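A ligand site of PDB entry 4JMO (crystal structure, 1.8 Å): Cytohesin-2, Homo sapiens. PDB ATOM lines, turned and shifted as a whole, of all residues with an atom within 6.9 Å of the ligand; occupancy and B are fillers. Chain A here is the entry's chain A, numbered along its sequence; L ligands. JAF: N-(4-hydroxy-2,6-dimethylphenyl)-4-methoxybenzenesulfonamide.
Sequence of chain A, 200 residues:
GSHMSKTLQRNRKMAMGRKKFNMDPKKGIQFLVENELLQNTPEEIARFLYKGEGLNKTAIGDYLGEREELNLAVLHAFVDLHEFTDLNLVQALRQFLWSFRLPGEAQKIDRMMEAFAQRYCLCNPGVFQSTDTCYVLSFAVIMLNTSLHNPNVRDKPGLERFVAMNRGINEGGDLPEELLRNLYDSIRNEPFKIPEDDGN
An oxygen (OAF) of the ligand lies within hydrogen-bond range of the backbone carbonyl oxygen (O) of Leu 97, 3.1 Å away.
The backbone NH (N) of Leu 102 is in hydrogen-bond range of an oxygen (OAF) of the ligand (3.2 Å).
O of Phe 100 lies within hydrogen-bond range of OAF of the ligand (3.0 Å).
Arg 101 touches the ligand (NH1 to CAL, 3.3 Å).
Ile 109 touches the ligand (CG2 to OAN, 3.8 Å).
CE1 of Phe 139 touches OAN of the ligand, 3.9 Å away.
CG2 of Ile 142 touches CAS of the ligand, at 3.3 Å.
Asn 145 touches the ligand.
OG1 of Thr 146 touches OAD of the ligand, 3.8 Å away.
CD2 of Phe 192 touches OAE of the ligand, 3.9 Å away.
Lys 193 touches the ligand.
CG1 of Ile 194 touches CAB of the ligand, 3.4 Å away.
Pro 195 touches the ligand (CD to CAK, 3.7 Å).
13 residues have an atom within 4 Å of the ligand: Leu 97, Phe 100, Arg 101, Leu 102, Ile 109, Phe 139, Ile 142, Asn 145, Thr 146, Phe 192, Lys 193, Ile 194 and Pro 195.
Along chain A the residues within 4 Å of the ligand span positions 97 to 195.
The nearest printed residue that does not touch the ligand is Trp 98 (5.3 Å).
N of Phe 192 lies close to ND2 of Asn 145 (2.9 Å).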
ATOM      1  N   PHE A  96      10.861   7.076  14.132  1.00  0.00           N
ATOM      2  CA  PHE A  96       9.469   6.589  14.193  1.00  0.00           C
ATOM      3  C   PHE A  96       8.617   7.472  15.083  1.00  0.00           C
ATOM      4  O   PHE A  96       7.506   7.924  14.732  1.00  0.00           O
ATOM      5  CB  PHE A  96       9.440   5.157  14.737  1.00  0.00           C
ATOM      6  CG  PHE A  96       8.062   4.521  14.758  1.00  0.00           C
ATOM      7  CD1 PHE A  96       7.416   4.286  13.558  1.00  0.00           C
ATOM      8  CD2 PHE A  96       7.426   4.188  15.956  1.00  0.00           C
ATOM      9  CE1 PHE A  96       6.176   3.678  13.527  1.00  0.00           C
ATOM     10  CE2 PHE A  96       6.168   3.587  15.938  1.00  0.00           C
ATOM     11  CZ  PHE A  96       5.544   3.332  14.724  1.00  0.00           C
ATOM     12  N   LEU A  97       9.149   7.729  16.276  1.00  0.00           N
ATOM     13  CA  LEU A  97       8.433   8.492  17.272  1.00  0.00           C
ATOM     14  C   LEU A  97       8.237   9.980  16.877  1.00  0.00           C
ATOM     15  O   LEU A  97       7.366  10.674  17.442  1.00  0.00           O
ATOM     16  CB  LEU A  97       9.163   8.384  18.617  1.00  0.00           C
ATOM     17  CG  LEU A  97       9.169   7.018  19.304  1.00  0.00           C
ATOM     18  CD1 LEU A  97      10.003   7.074  20.570  1.00  0.00           C
ATOM     19  CD2 LEU A  97       7.769   6.625  19.661  1.00  0.00           C
ATOM     20  N   TRP A  98       9.062  10.466  15.944  1.00  0.00           N
ATOM     21  CA  TRP A  98       8.917  11.831  15.433  1.00  0.00           C
ATOM     22  C   TRP A  98       7.792  11.931  14.400  1.00  0.00           C
ATOM     23  O   TRP A  98       7.201  13.011  14.212  1.00  0.00           O
ATOM     24  CB  TRP A  98      10.236  12.353  14.851  1.00  0.00           C
ATOM     25  CG  TRP A  98      10.166  13.824  14.413  1.00  0.00           C
ATOM     26  CD1 TRP A  98      10.179  14.291  13.128  1.00  0.00           C
ATOM     27  CD2 TRP A  98      10.062  14.972  15.260  1.00  0.00           C
ATOM     28  NE1 TRP A  98      10.103  15.667  13.135  1.00  0.00           N
ATOM     29  CE2 TRP A  98      10.016  16.104  14.433  1.00  0.00           C
ATOM     30  CE3 TRP A  98       9.964  15.150  16.642  1.00  0.00           C
ATOM     31  CZ2 TRP A  98       9.891  17.405  14.940  1.00  0.00           C
ATOM     32  CZ3 TRP A  98       9.866  16.430  17.150  1.00  0.00           C
ATOM     33  CH2 TRP A  98       9.819  17.549  16.305  1.00  0.00           C
ATOM     34  N   SER A  99       7.500  10.804  13.729  1.00  0.00           N
ATOM     35  CA  SER A  99       6.602  10.824  12.564  1.00  0.00           C
ATOM     36  C   SER A  99       5.113  11.036  12.926  1.00  0.00           C
ATOM     37  O   SER A  99       4.345  11.451  12.086  1.00  0.00           O
ATOM     38  CB  SER A  99       6.819   9.584  11.691  1.00  0.00           C
ATOM     39  OG  SER A  99       6.429   8.381  12.372  1.00  0.00           O
ATOM     40  N   PHE A 100       4.758  10.794  14.180  1.00  0.00           N
ATOM     41  CA  PHE A 100       3.432  11.031  14.697  1.00  0.00           C
ATOM     42  C   PHE A 100       3.504  11.037  16.196  1.00  0.00           C
ATOM     43  O   PHE A 100       4.516  10.634  16.789  1.00  0.00           O
ATOM     44  CB  PHE A 100       2.422   9.987  14.197  1.00  0.00           C
ATOM     45  CG  PHE A 100       2.666   8.598  14.694  1.00  0.00           C
ATOM     46  CD1 PHE A 100       3.702   7.840  14.188  1.00  0.00           C
ATOM     47  CD2 PHE A 100       1.866   8.044  15.684  1.00  0.00           C
ATOM     48  CE1 PHE A 100       3.931   6.543  14.644  1.00  0.00           C
ATOM     49  CE2 PHE A 100       2.090   6.760  16.142  1.00  0.00           C
ATOM     50  CZ  PHE A 100       3.115   6.015  15.622  1.00  0.00           C
ATOM     51  N   ARG A 101       2.451  11.500  16.806  1.00  0.00           N
ATOM     52  CA  ARG A 101       2.346  11.536  18.250  1.00  0.00           C
ATOM     53  C   ARG A 101       1.516  10.341  18.722  1.00  0.00           C
ATOM     54  O   ARG A 101       0.382  10.127  18.259  1.00  0.00           O
ATOM     55  CB  ARG A 101       1.781  12.874  18.695  1.00  0.00           C
ATOM     56  CG  ARG A 101       1.558  13.017  20.205  1.00  0.00           C
ATOM     57  CD  ARG A 101       2.871  13.237  20.934  1.00  0.00           C
ATOM     58  NE  ARG A 101       2.654  13.509  22.364  1.00  0.00           N
ATOM     59  CZ  ARG A 101       2.287  12.591  23.260  1.00  0.00           C
ATOM     60  NH1 ARG A 101       2.070  11.315  22.928  1.00  0.00           N
ATOM     61  NH2 ARG A 101       2.136  12.950  24.525  1.00  0.00           N
ATOM     62  N   LEU A 102       2.101   9.528  19.598  1.00  0.00           N
ATOM     63  CA  LEU A 102       1.432   8.324  20.052  1.00  0.00           C
ATOM     64  C   LEU A 102       0.125   8.683  20.706  1.00  0.00           C
ATOM     65  O   LEU A 102       0.060   9.664  21.447  1.00  0.00           O
ATOM     66  CB  LEU A 102       2.256   7.513  21.071  1.00  0.00           C
ATOM     67  CG  LEU A 102       3.481   6.782  20.525  1.00  0.00           C
ATOM     68  CD1 LEU A 102       4.366   6.250  21.640  1.00  0.00           C
ATOM     69  CD2 LEU A 102       3.061   5.635  19.650  1.00  0.00           C
ATOM     70  N   PRO A 103      -0.919   7.888  20.467  1.00  0.00           N
ATOM     71  CA  PRO A 103      -2.135   8.127  21.269  1.00  0.00           C
ATOM     72  C   PRO A 103      -1.948   7.675  22.707  1.00  0.00           C
ATOM     73  O   PRO A 103      -0.924   7.080  23.056  1.00  0.00           O
ATOM     74  CB  PRO A 103      -3.190   7.318  20.570  1.00  0.00           C
ATOM     75  CG  PRO A 103      -2.485   6.310  19.751  1.00  0.00           C
ATOM     76  CD  PRO A 103      -1.078   6.769  19.523  1.00  0.00           C
ATOM     77  N   GLY A 104      -2.941   7.963  23.549  1.00  0.00           N
ATOM     78  CA  GLY A 104      -2.837   7.669  24.961  1.00  0.00           C
ATOM     79  C   GLY A 104      -3.170   6.245  25.350  1.00  0.00           C
ATOM     80  O   GLY A 104      -2.769   5.786  26.409  1.00  0.00           O
ATOM     81  N   ILE A 109      -1.006   1.894  21.477  1.00  0.00           N
ATOM     82  CA  ILE A 109       0.444   2.014  21.565  1.00  0.00           C
ATOM     83  C   ILE A 109       1.066   0.614  21.356  1.00  0.00           C
ATOM     84  O   ILE A 109       2.069   0.445  20.648  1.00  0.00           O
ATOM     85  CB  ILE A 109       0.867   2.635  22.896  1.00  0.00           C
ATOM     86  CG1 ILE A 109       0.234   4.019  23.084  1.00  0.00           C
ATOM     87  CG2 ILE A 109       2.373   2.726  23.004  1.00  0.00           C
ATOM     88  CD1 ILE A 109       0.440   4.621  24.473  1.00  0.00           C
ATOM     89  N   MET A 113       3.876  -0.149  18.487  1.00  0.00           N
ATOM     90  CA  MET A 113       5.229  -0.555  18.852  1.00  0.00           C
ATOM     91  C   MET A 113       5.532  -1.965  18.374  1.00  0.00           C
ATOM     92  O   MET A 113       6.652  -2.265  17.990  1.00  0.00           O
ATOM     93  CB  MET A 113       5.450  -0.397  20.353  1.00  0.00           C
ATOM     94  CG  MET A 113       5.423   1.052  20.813  1.00  0.00           C
ATOM     95  SD  MET A 113       6.498   2.212  19.919  1.00  0.00           S
ATOM     96  CE  MET A 113       8.079   1.437  20.157  1.00  0.00           C
ATOM     97  N   PHE A 139      10.893  -0.427  24.589  1.00  0.00           N
ATOM     98  CA  PHE A 139      10.407   0.178  25.852  1.00  0.00           C
ATOM     99  C   PHE A 139      11.494   0.443  26.890  1.00  0.00           C
ATOM    100  O   PHE A 139      11.401   1.418  27.661  1.00  0.00           O
ATOM    101  CB  PHE A 139       9.219  -0.613  26.415  1.00  0.00           C
ATOM    102  CG  PHE A 139       7.940  -0.342  25.685  1.00  0.00           C
ATOM    103  CD1 PHE A 139       7.275   0.845  25.893  1.00  0.00           C
ATOM    104  CD2 PHE A 139       7.443  -1.240  24.740  1.00  0.00           C
ATOM    105  CE1 PHE A 139       6.105   1.130  25.221  1.00  0.00           C
ATOM    106  CE2 PHE A 139       6.270  -0.952  24.038  1.00  0.00           C
ATOM    107  CZ  PHE A 139       5.616   0.235  24.279  1.00  0.00           C
ATOM    108  N   VAL A 141      14.526   1.435  26.211  1.00  0.00           N
ATOM    109  CA  VAL A 141      15.070   2.712  25.739  1.00  0.00           C
ATOM    110  C   VAL A 141      14.163   3.911  26.052  1.00  0.00           C
ATOM    111  O   VAL A 141      14.621   4.984  26.479  1.00  0.00           O
ATOM    112  CB  VAL A 141      15.336   2.645  24.227  1.00  0.00           C
ATOM    113  CG1 VAL A 141      15.594   4.016  23.668  1.00  0.00           C
ATOM    114  CG2 VAL A 141      16.541   1.761  23.975  1.00  0.00           C
ATOM    115  N   ILE A 142      12.872   3.762  25.829  1.00  0.00           N
ATOM    116  CA  ILE A 142      11.932   4.830  26.133  1.00  0.00           C
ATOM    117  C   ILE A 142      11.963   5.120  27.624  1.00  0.00           C
ATOM    118  O   ILE A 142      11.926   6.271  28.024  1.00  0.00           O
ATOM    119  CB  ILE A 142      10.502   4.472  25.680  1.00  0.00           C
ATOM    120  CG1 ILE A 142      10.428   4.482  24.170  1.00  0.00           C
ATOM    121  CG2 ILE A 142       9.464   5.436  26.272  1.00  0.00           C
ATOM    122  CD1 ILE A 142       9.188   3.830  23.600  1.00  0.00           C
ATOM    123  N   MET A 143      12.019   4.068  28.442  1.00  0.00           N
ATOM    124  CA  MET A 143      12.043   4.230  29.907  1.00  0.00           C
ATOM    125  C   MET A 143      13.338   4.919  30.364  1.00  0.00           C
ATOM    126  O   MET A 143      13.313   5.771  31.247  1.00  0.00           O
ATOM    127  CB  MET A 143      11.865   2.859  30.596  1.00  0.00           C
ATOM    128  CG  MET A 143      10.466   2.264  30.503  1.00  0.00           C
ATOM    129  SD  MET A 143      10.462   0.466  30.831  1.00  0.00           S
ATOM    130  CE  MET A 143       8.908   0.117  30.092  1.00  0.00           C
ATOM    131  N   ASN A 145      15.195   7.019  28.547  1.00  0.00           N
ATOM    132  CA  ASN A 145      14.982   8.435  28.137  1.00  0.00           C
ATOM    133  C   ASN A 145      14.300   9.250  29.220  1.00  0.00           C
ATOM    134  O   ASN A 145      14.730  10.342  29.608  1.00  0.00           O
ATOM    135  CB  ASN A 145      14.115   8.501  26.893  1.00  0.00           C
ATOM    136  CG  ASN A 145      13.981   9.909  26.373  1.00  0.00           C
ATOM    137  OD1 ASN A 145      12.929  10.522  26.424  1.00  0.00           O
ATOM    138  ND2 ASN A 145      15.089  10.447  25.933  1.00  0.00           N
ATOM    139  N   THR A 146      13.215   8.718  29.719  1.00  0.00           N
ATOM    140  CA  THR A 146      12.535   9.364  30.822  1.00  0.00           C
ATOM    141  C   THR A 146      13.382   9.417  32.083  1.00  0.00           C
ATOM    142  O   THR A 146      13.422  10.430  32.766  1.00  0.00           O
ATOM    143  CB  THR A 146      11.229   8.619  31.116  1.00  0.00           C
ATOM    144  OG1 THR A 146      10.325   8.908  30.058  1.00  0.00           O
ATOM    145  CG2 THR A 146      10.610   9.052  32.450  1.00  0.00           C
ATOM    146  N   PHE A 192      15.109  11.866  23.359  1.00  0.00           N
ATOM    147  CA  PHE A 192      14.139  11.803  22.262  1.00  0.00           C
ATOM    148  C   PHE A 192      13.427  13.126  22.090  1.00  0.00           C
ATOM    149  O   PHE A 192      12.995  13.758  23.067  1.00  0.00           O
ATOM    150  CB  PHE A 192      13.069  10.714  22.482  1.00  0.00           C
ATOM    151  CG  PHE A 192      13.529   9.296  22.217  1.00  0.00           C
ATOM    152  CD1 PHE A 192      14.132   8.957  21.021  1.00  0.00           C
ATOM    153  CD2 PHE A 192      13.242   8.284  23.123  1.00  0.00           C
ATOM    154  CE1 PHE A 192      14.517   7.662  20.769  1.00  0.00           C
ATOM    155  CE2 PHE A 192      13.610   6.996  22.884  1.00  0.00           C
ATOM    156  CZ  PHE A 192      14.269   6.665  21.710  1.00  0.00           C
ATOM    157  N   LYS A 193      13.256  13.544  20.849  1.00  0.00           N
ATOM    158  CA  LYS A 193      12.354  14.687  20.621  1.00  0.00           C
ATOM    159  C   LYS A 193      10.876  14.205  20.455  1.00  0.00           C
ATOM    160  O   LYS A 193      10.603  13.334  19.605  1.00  0.00           O
ATOM    161  CB  LYS A 193      12.806  15.486  19.418  1.00  0.00           C
ATOM    162  CG  LYS A 193      13.981  16.419  19.698  1.00  0.00           C
ATOM    163  CD  LYS A 193      14.314  17.290  18.493  1.00  0.00           C
ATOM    164  CE  LYS A 193      14.772  16.476  17.285  1.00  0.00           C
ATOM    165  NZ  LYS A 193      13.717  16.198  16.258  1.00  0.00           N
ATOM    166  N   ILE A 194       9.977  14.772  21.281  1.00  0.00           N
ATOM    167  CA  ILE A 194       8.490  14.599  21.157  1.00  0.00           C
ATOM    168  C   ILE A 194       7.890  15.638  20.206  1.00  0.00           C
ATOM    169  O   ILE A 194       8.227  16.816  20.274  1.00  0.00           O
ATOM    170  CB  ILE A 194       7.717  14.787  22.495  1.00  0.00           C
ATOM    171  CG1 ILE A 194       8.312  13.966  23.638  1.00  0.00           C
ATOM    172  CG2 ILE A 194       6.237  14.409  22.338  1.00  0.00           C
ATOM    173  CD1 ILE A 194       7.716  14.306  24.992  1.00  0.00           C
ATOM    174  N   PRO A 195       6.968  15.200  19.335  1.00  0.00           N
ATOM    175  CA  PRO A 195       6.293  16.162  18.460  1.00  0.00           C
ATOM    176  C   PRO A 195       5.383  17.124  19.207  1.00  0.00           C
ATOM    177  O   PRO A 195       4.615  16.680  20.052  1.00  0.00           O
ATOM    178  CB  PRO A 195       5.439  15.262  17.546  1.00  0.00           C
ATOM    179  CG  PRO A 195       6.076  13.918  17.592  1.00  0.00           C
ATOM    180  CD  PRO A 195       6.693  13.796  18.967  1.00  0.00           C
HETATM  181  CAB JAF L   1       9.217  11.064  22.203  1.00  0.00           C
HETATM  182  CAO JAF L   1       7.813  10.758  22.193  1.00  0.00           C
HETATM  183  CAK JAF L   1       7.126  10.747  20.971  1.00  0.00           C
HETATM  184  CAQ JAF L   1       5.759  10.458  20.891  1.00  0.00           C
HETATM  185  OAF JAF L   1       5.215  10.425  19.651  1.00  0.00           O
HETATM  186  CAL JAF L   1       5.026  10.167  22.040  1.00  0.00           C
HETATM  187  CAP JAF L   1       5.670  10.181  23.291  1.00  0.00           C
HETATM  188  CAC JAF L   1       4.938   9.911  24.453  1.00  0.00           C
HETATM  189  CAT JAF L   1       7.053  10.479  23.346  1.00  0.00           C
HETATM  190  NAM JAF L   1       7.666  10.488  24.559  1.00  0.00           N
HETATM  191  SAU JAF L   1       8.517   9.024  25.070  1.00  0.00           S
HETATM  192  OAD JAF L   1       9.244   9.137  26.453  1.00  0.00           O
HETATM  193  OAE JAF L   1       9.484   8.606  23.938  1.00  0.00           O
HETATM  194  CAS JAF L   1       7.364   7.830  25.239  1.00  0.00           C
HETATM  195  CAI JAF L   1       7.223   6.948  24.178  1.00  0.00           C
HETATM  196  CAG JAF L   1       6.278   5.944  24.290  1.00  0.00           C
HETATM  197  CAR JAF L   1       5.500   5.804  25.436  1.00  0.00           C
HETATM  198  OAN JAF L   1       4.595   4.755  25.390  1.00  0.00           O
HETATM  199  CAA JAF L   1       3.857   4.450  26.572  1.00  0.00           C
HETATM  200  CAH JAF L   1       5.650   6.718  26.507  1.00  0.00           C
HETATM  201  CAJ JAF L   1       6.591   7.728  26.403  1.00  0.00           C
